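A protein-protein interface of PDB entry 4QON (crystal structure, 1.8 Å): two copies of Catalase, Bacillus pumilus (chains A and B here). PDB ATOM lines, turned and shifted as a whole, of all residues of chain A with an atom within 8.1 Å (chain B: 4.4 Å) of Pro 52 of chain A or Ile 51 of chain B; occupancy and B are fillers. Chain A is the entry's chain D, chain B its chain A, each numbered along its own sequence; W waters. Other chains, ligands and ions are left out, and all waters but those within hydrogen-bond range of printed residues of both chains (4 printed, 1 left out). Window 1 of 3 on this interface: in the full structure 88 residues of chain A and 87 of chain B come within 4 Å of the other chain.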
ATOM      1  N   GLU A  49      -1.819  -2.542  13.012  1.00  0.00           N
ATOM      2  CA  GLU A  49      -0.347  -2.494  13.144  1.00  0.00           C
ATOM      3  C   GLU A  49       0.197  -3.270  14.368  1.00  0.00           C
ATOM      4  O   GLU A  49       1.268  -3.874  14.262  1.00  0.00           O
ATOM      5  CB  GLU A  49       0.169  -1.071  13.235  1.00  0.00           C
ATOM      6  CG  GLU A  49       0.065  -0.326  11.936  1.00  0.00           C
ATOM      7  CD  GLU A  49       0.714   1.053  11.895  1.00  0.00           C
ATOM      8  OE1 GLU A  49       0.530   1.752  10.899  1.00  0.00           O
ATOM      9  OE2 GLU A  49       1.341   1.443  12.873  1.00  0.00           O
ATOM     10  N   ARG A  50      -0.546  -3.259  15.480  1.00  0.00           N
ATOM     11  CA  ARG A  50      -0.015  -3.713  16.756  1.00  0.00           C
ATOM     12  C   ARG A  50      -0.258  -5.216  16.978  1.00  0.00           C
ATOM     13  O   ARG A  50      -1.318  -5.736  16.690  1.00  0.00           O
ATOM     14  CB  ARG A  50      -0.638  -2.949  17.916  1.00  0.00           C
ATOM     15  CG  ARG A  50      -0.467  -1.448  17.849  1.00  0.00           C
ATOM     16  CD  ARG A  50       1.010  -0.976  18.042  1.00  0.00           C
ATOM     17  NE  ARG A  50       0.962   0.440  17.819  1.00  0.00           N
ATOM     18  CZ  ARG A  50       1.286   1.072  16.710  1.00  0.00           C
ATOM     19  NH1 ARG A  50       1.813   0.468  15.660  1.00  0.00           N
ATOM     20  NH2 ARG A  50       1.026   2.362  16.628  1.00  0.00           N
ATOM     21  N   ILE A  51       0.729  -5.851  17.569  1.00  0.00           N
ATOM     22  CA  ILE A  51       0.625  -7.212  18.019  1.00  0.00           C
ATOM     23  C   ILE A  51       0.830  -7.244  19.534  1.00  0.00           C
ATOM     24  O   ILE A  51       1.293  -6.245  20.113  1.00  0.00           O
ATOM     25  CB  ILE A  51       1.601  -8.120  17.272  1.00  0.00           C
ATOM     26  CG1 ILE A  51       3.071  -7.798  17.573  1.00  0.00           C
ATOM     27  CG2 ILE A  51       1.381  -7.996  15.769  1.00  0.00           C
ATOM     28  CD1 ILE A  51       4.059  -8.753  16.956  1.00  0.00           C
ATOM     29  N   PRO A  52       0.474  -8.341  20.197  1.00  0.00           N
ATOM     30  CA  PRO A  52       0.791  -8.407  21.649  1.00  0.00           C
ATOM     31  C   PRO A  52       2.274  -8.239  21.961  1.00  0.00           C
ATOM     32  O   PRO A  52       3.112  -8.641  21.205  1.00  0.00           O
ATOM     33  CB  PRO A  52       0.257  -9.755  22.075  1.00  0.00           C
ATOM     34  CG  PRO A  52      -0.640 -10.224  20.951  1.00  0.00           C
ATOM     35  CD  PRO A  52      -0.014  -9.639  19.705  1.00  0.00           C
ATOM     36  N   GLU A  53       2.611  -7.551  23.050  1.00  0.00           N
ATOM     37  CA  GLU A  53       3.990  -7.391  23.450  1.00  0.00           C
ATOM     38  C   GLU A  53       4.375  -8.666  24.155  1.00  0.00           C
ATOM     39  O   GLU A  53       3.476  -9.454  24.546  1.00  0.00           O
ATOM     40  CB  GLU A  53       4.169  -6.169  24.373  1.00  0.00           C
ATOM     41  CG  GLU A  53       3.652  -6.331  25.785  1.00  0.00           C
ATOM     42  CD  GLU A  53       3.759  -5.074  26.646  1.00  0.00           C
ATOM     43  OE1 GLU A  53       3.979  -3.935  26.114  1.00  0.00           O
ATOM     44  OE2 GLU A  53       3.610  -5.266  27.907  1.00  0.00           O
ATOM     45  N   ARG A  54       5.664  -8.853  24.411  1.00  0.00           N
ATOM     46  CA  ARG A  54       6.129  -9.996  25.181  1.00  0.00           C
ATOM     47  C   ARG A  54       5.527  -9.990  26.614  1.00  0.00           C
ATOM     48  O   ARG A  54       5.440  -8.923  27.262  1.00  0.00           O
ATOM     49  CB  ARG A  54       7.641  -9.987  25.226  1.00  0.00           C
ATOM     50  CG  ARG A  54       8.387 -10.164  23.930  1.00  0.00           C
ATOM     51  CD  ARG A  54       9.809  -9.686  24.064  1.00  0.00           C
ATOM     52  NE  ARG A  54      10.580  -9.908  22.855  1.00  0.00           N
ATOM     53  CZ  ARG A  54      10.441  -9.277  21.700  1.00  0.00           C
ATOM     54  NH1 ARG A  54       9.623  -8.256  21.579  1.00  0.00           N
ATOM     55  NH2 ARG A  54      11.189  -9.655  20.637  1.00  0.00           N
ATOM     56  N   VAL A  55       5.049 -11.141  27.092  1.00  0.00           N
ATOM     57  CA  VAL A  55       4.485 -11.214  28.461  1.00  0.00           C
ATOM     58  C   VAL A  55       5.423 -10.764  29.560  1.00  0.00           C
ATOM     59  O   VAL A  55       5.009 -10.212  30.603  1.00  0.00           O
ATOM     60  CB  VAL A  55       3.906 -12.646  28.706  1.00  0.00           C
ATOM     61  CG1 VAL A  55       5.037 -13.631  28.854  1.00  0.00           C
ATOM     62  CG2 VAL A  55       2.985 -12.708  29.922  1.00  0.00           C
ATOM     63  N   ALA A  58       9.171  -6.981  27.801  1.00  0.00           N
ATOM     64  CA  ALA A  58       8.515  -6.262  26.719  1.00  0.00           C
ATOM     65  C   ALA A  58       9.316  -5.064  26.190  1.00  0.00           C
ATOM     66  O   ALA A  58       9.274  -4.756  24.979  1.00  0.00           O
ATOM     67  CB  ALA A  58       7.112  -5.826  27.160  1.00  0.00           C
ATOM     68  N   LYS A 102       6.038  -2.272  27.174  1.00  0.00           N
ATOM     69  CA  LYS A 102       6.859  -1.742  26.097  1.00  0.00           C
ATOM     70  C   LYS A 102       7.461  -0.347  26.225  1.00  0.00           C
ATOM     71  O   LYS A 102       8.600  -0.154  25.838  1.00  0.00           O
ATOM     72  CB  LYS A 102       6.054  -1.777  24.786  1.00  0.00           C
ATOM     73  CG  LYS A 102       6.468  -2.921  23.947  1.00  0.00           C
ATOM     74  CD  LYS A 102       5.700  -2.919  22.638  1.00  0.00           C
ATOM     75  CE  LYS A 102       6.206  -1.899  21.613  1.00  0.00           C
ATOM     76  NZ  LYS A 102       7.541  -2.265  21.015  1.00  0.00           N
ATOM     77  N   PHE A 308      10.302  -2.889  14.279  1.00  0.00           N
ATOM     78  CA  PHE A 308       9.148  -3.818  14.497  1.00  0.00           C
ATOM     79  C   PHE A 308       9.424  -5.153  13.857  1.00  0.00           C
ATOM     80  O   PHE A 308       9.249  -6.222  14.481  1.00  0.00           O
ATOM     81  CB  PHE A 308       7.867  -3.302  13.895  1.00  0.00           C
ATOM     82  CG  PHE A 308       6.725  -4.312  13.948  1.00  0.00           C
ATOM     83  CD1 PHE A 308       5.922  -4.385  15.044  1.00  0.00           C
ATOM     84  CD2 PHE A 308       6.466  -5.167  12.881  1.00  0.00           C
ATOM     85  CE1 PHE A 308       4.822  -5.294  15.131  1.00  0.00           C
ATOM     86  CE2 PHE A 308       5.427  -6.075  12.946  1.00  0.00           C
ATOM     87  CZ  PHE A 308       4.586  -6.144  14.064  1.00  0.00           C
ATOM     88  N   GLU A 312      11.060  -6.331  17.339  1.00  0.00           N
ATOM     89  CA  GLU A 312       9.819  -6.624  18.090  1.00  0.00           C
ATOM     90  C   GLU A 312       9.406  -8.043  17.789  1.00  0.00           C
ATOM     91  O   GLU A 312       8.974  -8.748  18.663  1.00  0.00           O
ATOM     92  CB  GLU A 312       8.721  -5.598  17.830  1.00  0.00           C
ATOM     93  CG  GLU A 312       7.432  -5.853  18.622  1.00  0.00           C
ATOM     94  CD  GLU A 312       7.570  -5.664  20.128  1.00  0.00           C
ATOM     95  OE1 GLU A 312       6.774  -6.281  20.860  1.00  0.00           O
ATOM     96  OE2 GLU A 312       8.441  -4.895  20.569  1.00  0.00           O
ATOM     97  N   GLN A 313       9.622  -8.491  16.548  1.00  0.00           N
ATOM     98  CA  GLN A 313       9.179  -9.840  16.123  1.00  0.00           C
ATOM     99  C   GLN A 313      10.226 -10.917  16.415  1.00  0.00           C
ATOM    100  O   GLN A 313       9.956 -12.057  16.165  1.00  0.00           O
ATOM    101  CB  GLN A 313       8.891  -9.849  14.634  1.00  0.00           C
ATOM    102  CG  GLN A 313       7.570  -9.165  14.211  1.00  0.00           C
ATOM    103  CD  GLN A 313       7.115  -9.481  12.799  1.00  0.00           C
ATOM    104  OE1 GLN A 313       5.969  -9.821  12.550  1.00  0.00           O
ATOM    105  NE2 GLN A 313       8.034  -9.361  11.848  1.00  0.00           N
ATOM    106  N   THR A 343       4.375 -19.304  23.798  1.00  0.00           N
ATOM    107  CA  THR A 343       4.061 -17.858  23.738  1.00  0.00           C
ATOM    108  C   THR A 343       4.299 -17.245  22.368  1.00  0.00           C
ATOM    109  O   THR A 343       3.505 -16.388  21.947  1.00  0.00           O
ATOM    110  CB  THR A 343       4.771 -17.022  24.836  1.00  0.00           C
ATOM    111  OG1 THR A 343       3.974 -15.858  25.140  1.00  0.00           O
ATOM    112  CG2 THR A 343       6.165 -16.603  24.409  1.00  0.00           C
ATOM    113  N   HIS A 346       1.456 -17.715  19.766  1.00  0.00           N
ATOM    114  CA  HIS A 346       0.385 -16.737  20.080  1.00  0.00           C
ATOM    115  C   HIS A 346       0.778 -15.336  19.663  1.00  0.00           C
ATOM    116  O   HIS A 346       0.000 -14.650  18.956  1.00  0.00           O
ATOM    117  CB  HIS A 346       0.132 -16.792  21.589  1.00  0.00           C
ATOM    118  CG  HIS A 346      -0.584 -15.609  22.135  1.00  0.00           C
ATOM    119  ND1 HIS A 346      -1.881 -15.316  21.808  1.00  0.00           N
ATOM    120  CD2 HIS A 346      -0.188 -14.666  23.022  1.00  0.00           C
ATOM    121  CE1 HIS A 346      -2.257 -14.240  22.474  1.00  0.00           C
ATOM    122  NE2 HIS A 346      -1.238 -13.817  23.195  1.00  0.00           N
ATOM    123  N   ARG A 347       2.000 -14.910  20.058  1.00  0.00           N
ATOM    124  CA  ARG A 347       2.447 -13.517  19.917  1.00  0.00           C
ATOM    125  C   ARG A 347       2.686 -13.187  18.423  1.00  0.00           C
ATOM    126  O   ARG A 347       2.316 -12.114  17.957  1.00  0.00           O
ATOM    127  CB  ARG A 347       3.717 -13.246  20.712  1.00  0.00           C
ATOM    128  CG  ARG A 347       4.207 -11.819  20.652  1.00  0.00           C
ATOM    129  CD  ARG A 347       5.273 -11.536  21.649  1.00  0.00           C
ATOM    130  NE  ARG A 347       6.560 -12.235  21.493  1.00  0.00           N
ATOM    131  CZ  ARG A 347       7.575 -11.825  20.707  1.00  0.00           C
ATOM    132  NH1 ARG A 347       7.444 -10.748  19.888  1.00  0.00           N
ATOM    133  NH2 ARG A 347       8.735 -12.517  20.681  1.00  0.00           N
ATOM    134  N   LEU A 348       3.218 -14.152  17.680  1.00  0.00           N
ATOM    135  CA  LEU A 348       3.734 -13.894  16.321  1.00  0.00           C
ATOM    136  C   LEU A 348       3.056 -14.681  15.182  1.00  0.00           C
ATOM    137  O   LEU A 348       3.169 -14.256  14.017  1.00  0.00           O
ATOM    138  CB  LEU A 348       5.220 -14.220  16.292  1.00  0.00           C
ATOM    139  CG  LEU A 348       6.049 -13.363  17.217  1.00  0.00           C
ATOM    140  CD1 LEU A 348       7.440 -13.980  17.359  1.00  0.00           C
ATOM    141  CD2 LEU A 348       6.139 -11.903  16.706  1.00  0.00           C
ATOM    142  N   GLY A 349       2.348 -15.770  15.535  1.00  0.00           N
ATOM    143  CA  GLY A 349       1.708 -16.641  14.561  1.00  0.00           C
ATOM    144  C   GLY A 349       2.376 -17.988  14.479  1.00  0.00           C
ATOM    145  O   GLY A 349       3.556 -18.152  14.803  1.00  0.00           O
ATOM    146  N   GLU B  49      -1.567 -14.184  28.112  1.00  0.00           N
ATOM    147  CA  GLU B  49      -2.230 -13.086  28.785  1.00  0.00           C
ATOM    148  C   GLU B  49      -2.383 -11.769  27.992  1.00  0.00           C
ATOM    149  O   GLU B  49      -3.402 -11.070  28.146  1.00  0.00           O
ATOM    150  CB  GLU B  49      -1.507 -12.728  30.075  1.00  0.00           C
ATOM    151  CG  GLU B  49      -1.588 -13.781  31.100  1.00  0.00           C
ATOM    152  CD  GLU B  49      -0.974 -13.446  32.419  1.00  0.00           C
ATOM    153  OE1 GLU B  49      -0.879 -14.298  33.312  1.00  0.00           O
ATOM    154  OE2 GLU B  49      -0.589 -12.335  32.644  1.00  0.00           O
ATOM    155  N   ARG B  50      -1.417 -11.466  27.139  1.00  0.00           N
ATOM    156  CA  ARG B  50      -1.336 -10.137  26.501  1.00  0.00           C
ATOM    157  C   ARG B  50      -2.040 -10.048  25.198  1.00  0.00           C
ATOM    158  O   ARG B  50      -2.051 -10.991  24.382  1.00  0.00           O
ATOM    159  CB  ARG B  50       0.128  -9.786  26.247  1.00  0.00           C
ATOM    160  CG  ARG B  50       1.019  -9.761  27.456  1.00  0.00           C
ATOM    161  CD  ARG B  50       0.662  -8.656  28.487  1.00  0.00           C
ATOM    162  NE  ARG B  50       1.540  -8.914  29.598  1.00  0.00           N
ATOM    163  CZ  ARG B  50       1.223  -9.558  30.710  1.00  0.00           C
ATOM    164  NH1 ARG B  50      -0.025  -9.932  30.982  1.00  0.00           N
ATOM    165  NH2 ARG B  50       2.164  -9.743  31.608  1.00  0.00           N
ATOM    166  N   ILE B  51      -2.724  -8.946  25.028  1.00  0.00           N
ATOM    167  CA  ILE B  51      -3.373  -8.598  23.778  1.00  0.00           C
ATOM    168  C   ILE B  51      -2.738  -7.327  23.165  1.00  0.00           C
ATOM    169  O   ILE B  51      -2.021  -6.587  23.874  1.00  0.00           O
ATOM    170  CB  ILE B  51      -4.889  -8.424  23.915  1.00  0.00           C
ATOM    171  CG1 ILE B  51      -5.269  -7.220  24.817  1.00  0.00           C
ATOM    172  CG2 ILE B  51      -5.471  -9.674  24.517  1.00  0.00           C
ATOM    173  CD1 ILE B  51      -6.767  -6.981  24.874  1.00  0.00           C
ATOM    174  N   PRO B  52      -2.979  -7.058  21.867  1.00  0.00           N
ATOM    175  CA  PRO B  52      -2.371  -5.857  21.325  1.00  0.00           C
ATOM    176  C   PRO B  52      -2.837  -4.589  22.061  1.00  0.00           C
ATOM    177  O   PRO B  52      -3.937  -4.534  22.528  1.00  0.00           O
ATOM    178  CB  PRO B  52      -2.824  -5.831  19.852  1.00  0.00           C
ATOM    179  CG  PRO B  52      -3.219  -7.222  19.564  1.00  0.00           C
ATOM    180  CD  PRO B  52      -3.800  -7.747  20.856  1.00  0.00           C
ATOM    181  N   GLU B  53      -1.927  -3.642  22.276  1.00  0.00           N
ATOM    182  CA  GLU B  53      -2.314  -2.402  22.951  1.00  0.00           C
ATOM    183  C   GLU B  53      -3.056  -1.574  21.900  1.00  0.00           C
ATOM    184  O   GLU B  53      -2.939  -1.823  20.679  1.00  0.00           O
ATOM    185  CB  GLU B  53      -1.108  -1.638  23.560  1.00  0.00           C
ATOM    186  CG  GLU B  53      -0.216  -0.942  22.536  1.00  0.00           C
ATOM    187  CD  GLU B  53       1.003  -0.294  23.128  1.00  0.00           C
ATOM    188  OE1 GLU B  53       1.382  -0.545  24.316  1.00  0.00           O
ATOM    189  OE2 GLU B  53       1.612   0.510  22.356  1.00  0.00           O
ATOM    190  N   PHE B 308      -7.213  -4.919  33.555  1.00  0.00           N
ATOM    191  CA  PHE B 308      -7.221  -5.535  32.188  1.00  0.00           C
ATOM    192  C   PHE B 308      -8.649  -5.735  31.654  1.00  0.00           C
ATOM    193  O   PHE B 308      -8.965  -5.342  30.529  1.00  0.00           O
ATOM    194  CB  PHE B 308      -6.537  -6.860  32.199  1.00  0.00           C
ATOM    195  CG  PHE B 308      -6.583  -7.586  30.861  1.00  0.00           C
ATOM    196  CD1 PHE B 308      -5.627  -7.344  29.919  1.00  0.00           C
ATOM    197  CD2 PHE B 308      -7.628  -8.459  30.575  1.00  0.00           C
ATOM    198  CE1 PHE B 308      -5.678  -8.003  28.641  1.00  0.00           C
ATOM    199  CE2 PHE B 308      -7.727  -9.102  29.254  1.00  0.00           C
ATOM    200  CZ  PHE B 308      -6.734  -8.853  28.344  1.00  0.00           C
ATOM    201  N   ARG B 347      -8.266  -5.845  17.890  1.00  0.00           N
ATOM    202  CA  ARG B 347      -7.633  -5.753  19.219  1.00  0.00           C
ATOM    203  C   ARG B 347      -8.285  -6.699  20.212  1.00  0.00           C
ATOM    204  O   ARG B 347      -7.610  -7.290  21.058  1.00  0.00           O
ATOM    205  CB  ARG B 347      -7.667  -4.286  19.708  1.00  0.00           C
ATOM    206  CG  ARG B 347      -7.008  -4.047  21.059  1.00  0.00           C
ATOM    207  CD  ARG B 347      -6.847  -2.598  21.398  1.00  0.00           C
ATOM    208  NE  ARG B 347      -8.048  -1.781  21.666  1.00  0.00           N
ATOM    209  CZ  ARG B 347      -8.708  -1.735  22.824  1.00  0.00           C
ATOM    210  NH1 ARG B 347      -8.336  -2.475  23.868  1.00  0.00           N
ATOM    211  NH2 ARG B 347      -9.767  -0.945  22.945  1.00  0.00           N
ATOM    212  N   LEU B 348      -9.630  -6.820  20.142  1.00  0.00           N
ATOM    213  CA  LEU B 348     -10.428  -7.420  21.216  1.00  0.00           C
ATOM    214  C   LEU B 348     -11.214  -8.677  20.796  1.00  0.00           C
ATOM    215  O   LEU B 348     -11.617  -9.446  21.690  1.00  0.00           O
ATOM    216  CB  LEU B 348     -11.436  -6.414  21.794  1.00  0.00           C
ATOM    217  CG  LEU B 348     -10.785  -5.208  22.464  1.00  0.00           C
ATOM    218  CD1 LEU B 348     -11.837  -4.117  22.670  1.00  0.00           C
ATOM    219  CD2 LEU B 348     -10.122  -5.605  23.777  1.00  0.00           C
HETATM  220  O   HOH W   1       0.917  -4.299  21.868  1.00  0.00           O
HETATM  221  O   HOH W   2       2.064  -3.177  24.497  1.00  0.00           O
HETATM  222  O   HOH W   3       0.421   1.941  20.303  1.00  0.00           O
HETATM  223  O   HOH W   4       0.574  -5.941  24.530  1.00  0.00           O
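Of the printed residues of chain B, Arg 50 of chain A touches Pro 52 and Glu 53.
Of the printed residues of chain B, Ile 51 of chain A touches Pro 52 (3.9 Å).
Printed residues of chain B within 4 Å of Pro 52 of chain A: Arg 50 (3.5 Å), Ile 51 (3.99 Å) and Pro 52 (3.9 Å).
Of the printed residues of chain B, Glu 53 of chain A touches Arg 50.
Printed residues of chain A within 4 Å of Ile 51 of chain B: Pro 52.
Pro 52 of chain B touches just these residues of chain A: Arg 50, Ile 51 and Pro 52.
Printed residues of chain A within 4 Å of Glu 53 of chain B: Arg 50.
The nearest printed residue of chain B that does not touch Pro 52 of chain A is Glu 53 of chain B (5.5 Å).
The nearest printed residue of chain A that does not touch Ile 51 of chain B is Glu 53 of chain A (4.8 Å).
The nearest printed residue of chain B that does not touch Arg 50 of chain A is Arg 347 of chain B (6.8 Å).
Water W2 bridges OE1 of Glu 53 of chain A and OE1 of Glu 53 of chain B.
Water W1 lies within hydrogen-bond range of the backbone carbonyl oxygen (O) of Ile 51 of chain A (2.6 Å) and the backbone NH (N) of Glu 53 of chain B (2.9 Å).
Water W4 bridges O of Ile 51 of chain B (2.8 Å) and N of Glu 53 of chain A (3.0 Å).
Water W3 lies within hydrogen-bond range of OE2 of Glu 53 of chain B and NE of Arg 50 of chain A.
Hydrophobic or aromatic side chains of chain B within 4 Å of the printed part of chain A: Pro 52.
Among the printed residues, 9 pairs touch across the chains.
Among the printed residues, no Asp or Glu carboxylate lies within 4 Å of a Lys or Arg side-chain nitrogen of the other chain.
Arg 50 of chain A touches Pro 52 of chain B, and with the chains exchanged Pro 52 of chain A touches Arg 50 of chain B.
Arg 50 of chain A touches Glu 53 of chain B, and with the chains exchanged Glu 53 of chain A touches Arg 50 of chain B.
Ile 51 of chain A touches Pro 52 of chain B, and with the chains exchanged Pro 52 of chain A touches Ile 51 of chain B.
Pro 52 of chain B touches its own counterpart, Pro 52 of chain A.
Positions printed for both chains: 49, 50, 51, 52, 53, 308, 347 and 348.
Among the printed residues, merely in contact across the chains: Pro 52 of chain A with Arg 50 of chain B, Arg 50 of chain A with Pro 52 of chain B, Arg 50 of chain A with Glu 53 of chain B, Glu 53 of chain A with Arg 50 of chain B, Ile 51 of chain A with Pro 52 of chain B, Pro 52 of chain A with Pro 52 of chain B and Pro 52 of chain A with Ile 51 of chain B.
O of Val 55 of chain A sits at hydrogen-bond distance from NH2 of Arg 50 of chain B, at 3.1 Å.
The backbone carbonyl oxygen (O) of Arg 50 of chain B lies within hydrogen-bond range of a ring nitrogen (NE2) of His 346 of chain A (3.2 Å).
OE2 of Glu 49 of chain A is in salt-bridge range of NH1 of Arg 50 of chain A, 3.0 Å away.
OE1 of Glu 53 of chain A lies within hydrogen-bond range of N of Lys 102 of chain A (2.9 Å).
OE2 of Glu 49 of chain B lies within salt-bridge range of NH1 of Arg 50 of chain B, at 3.0 Å.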
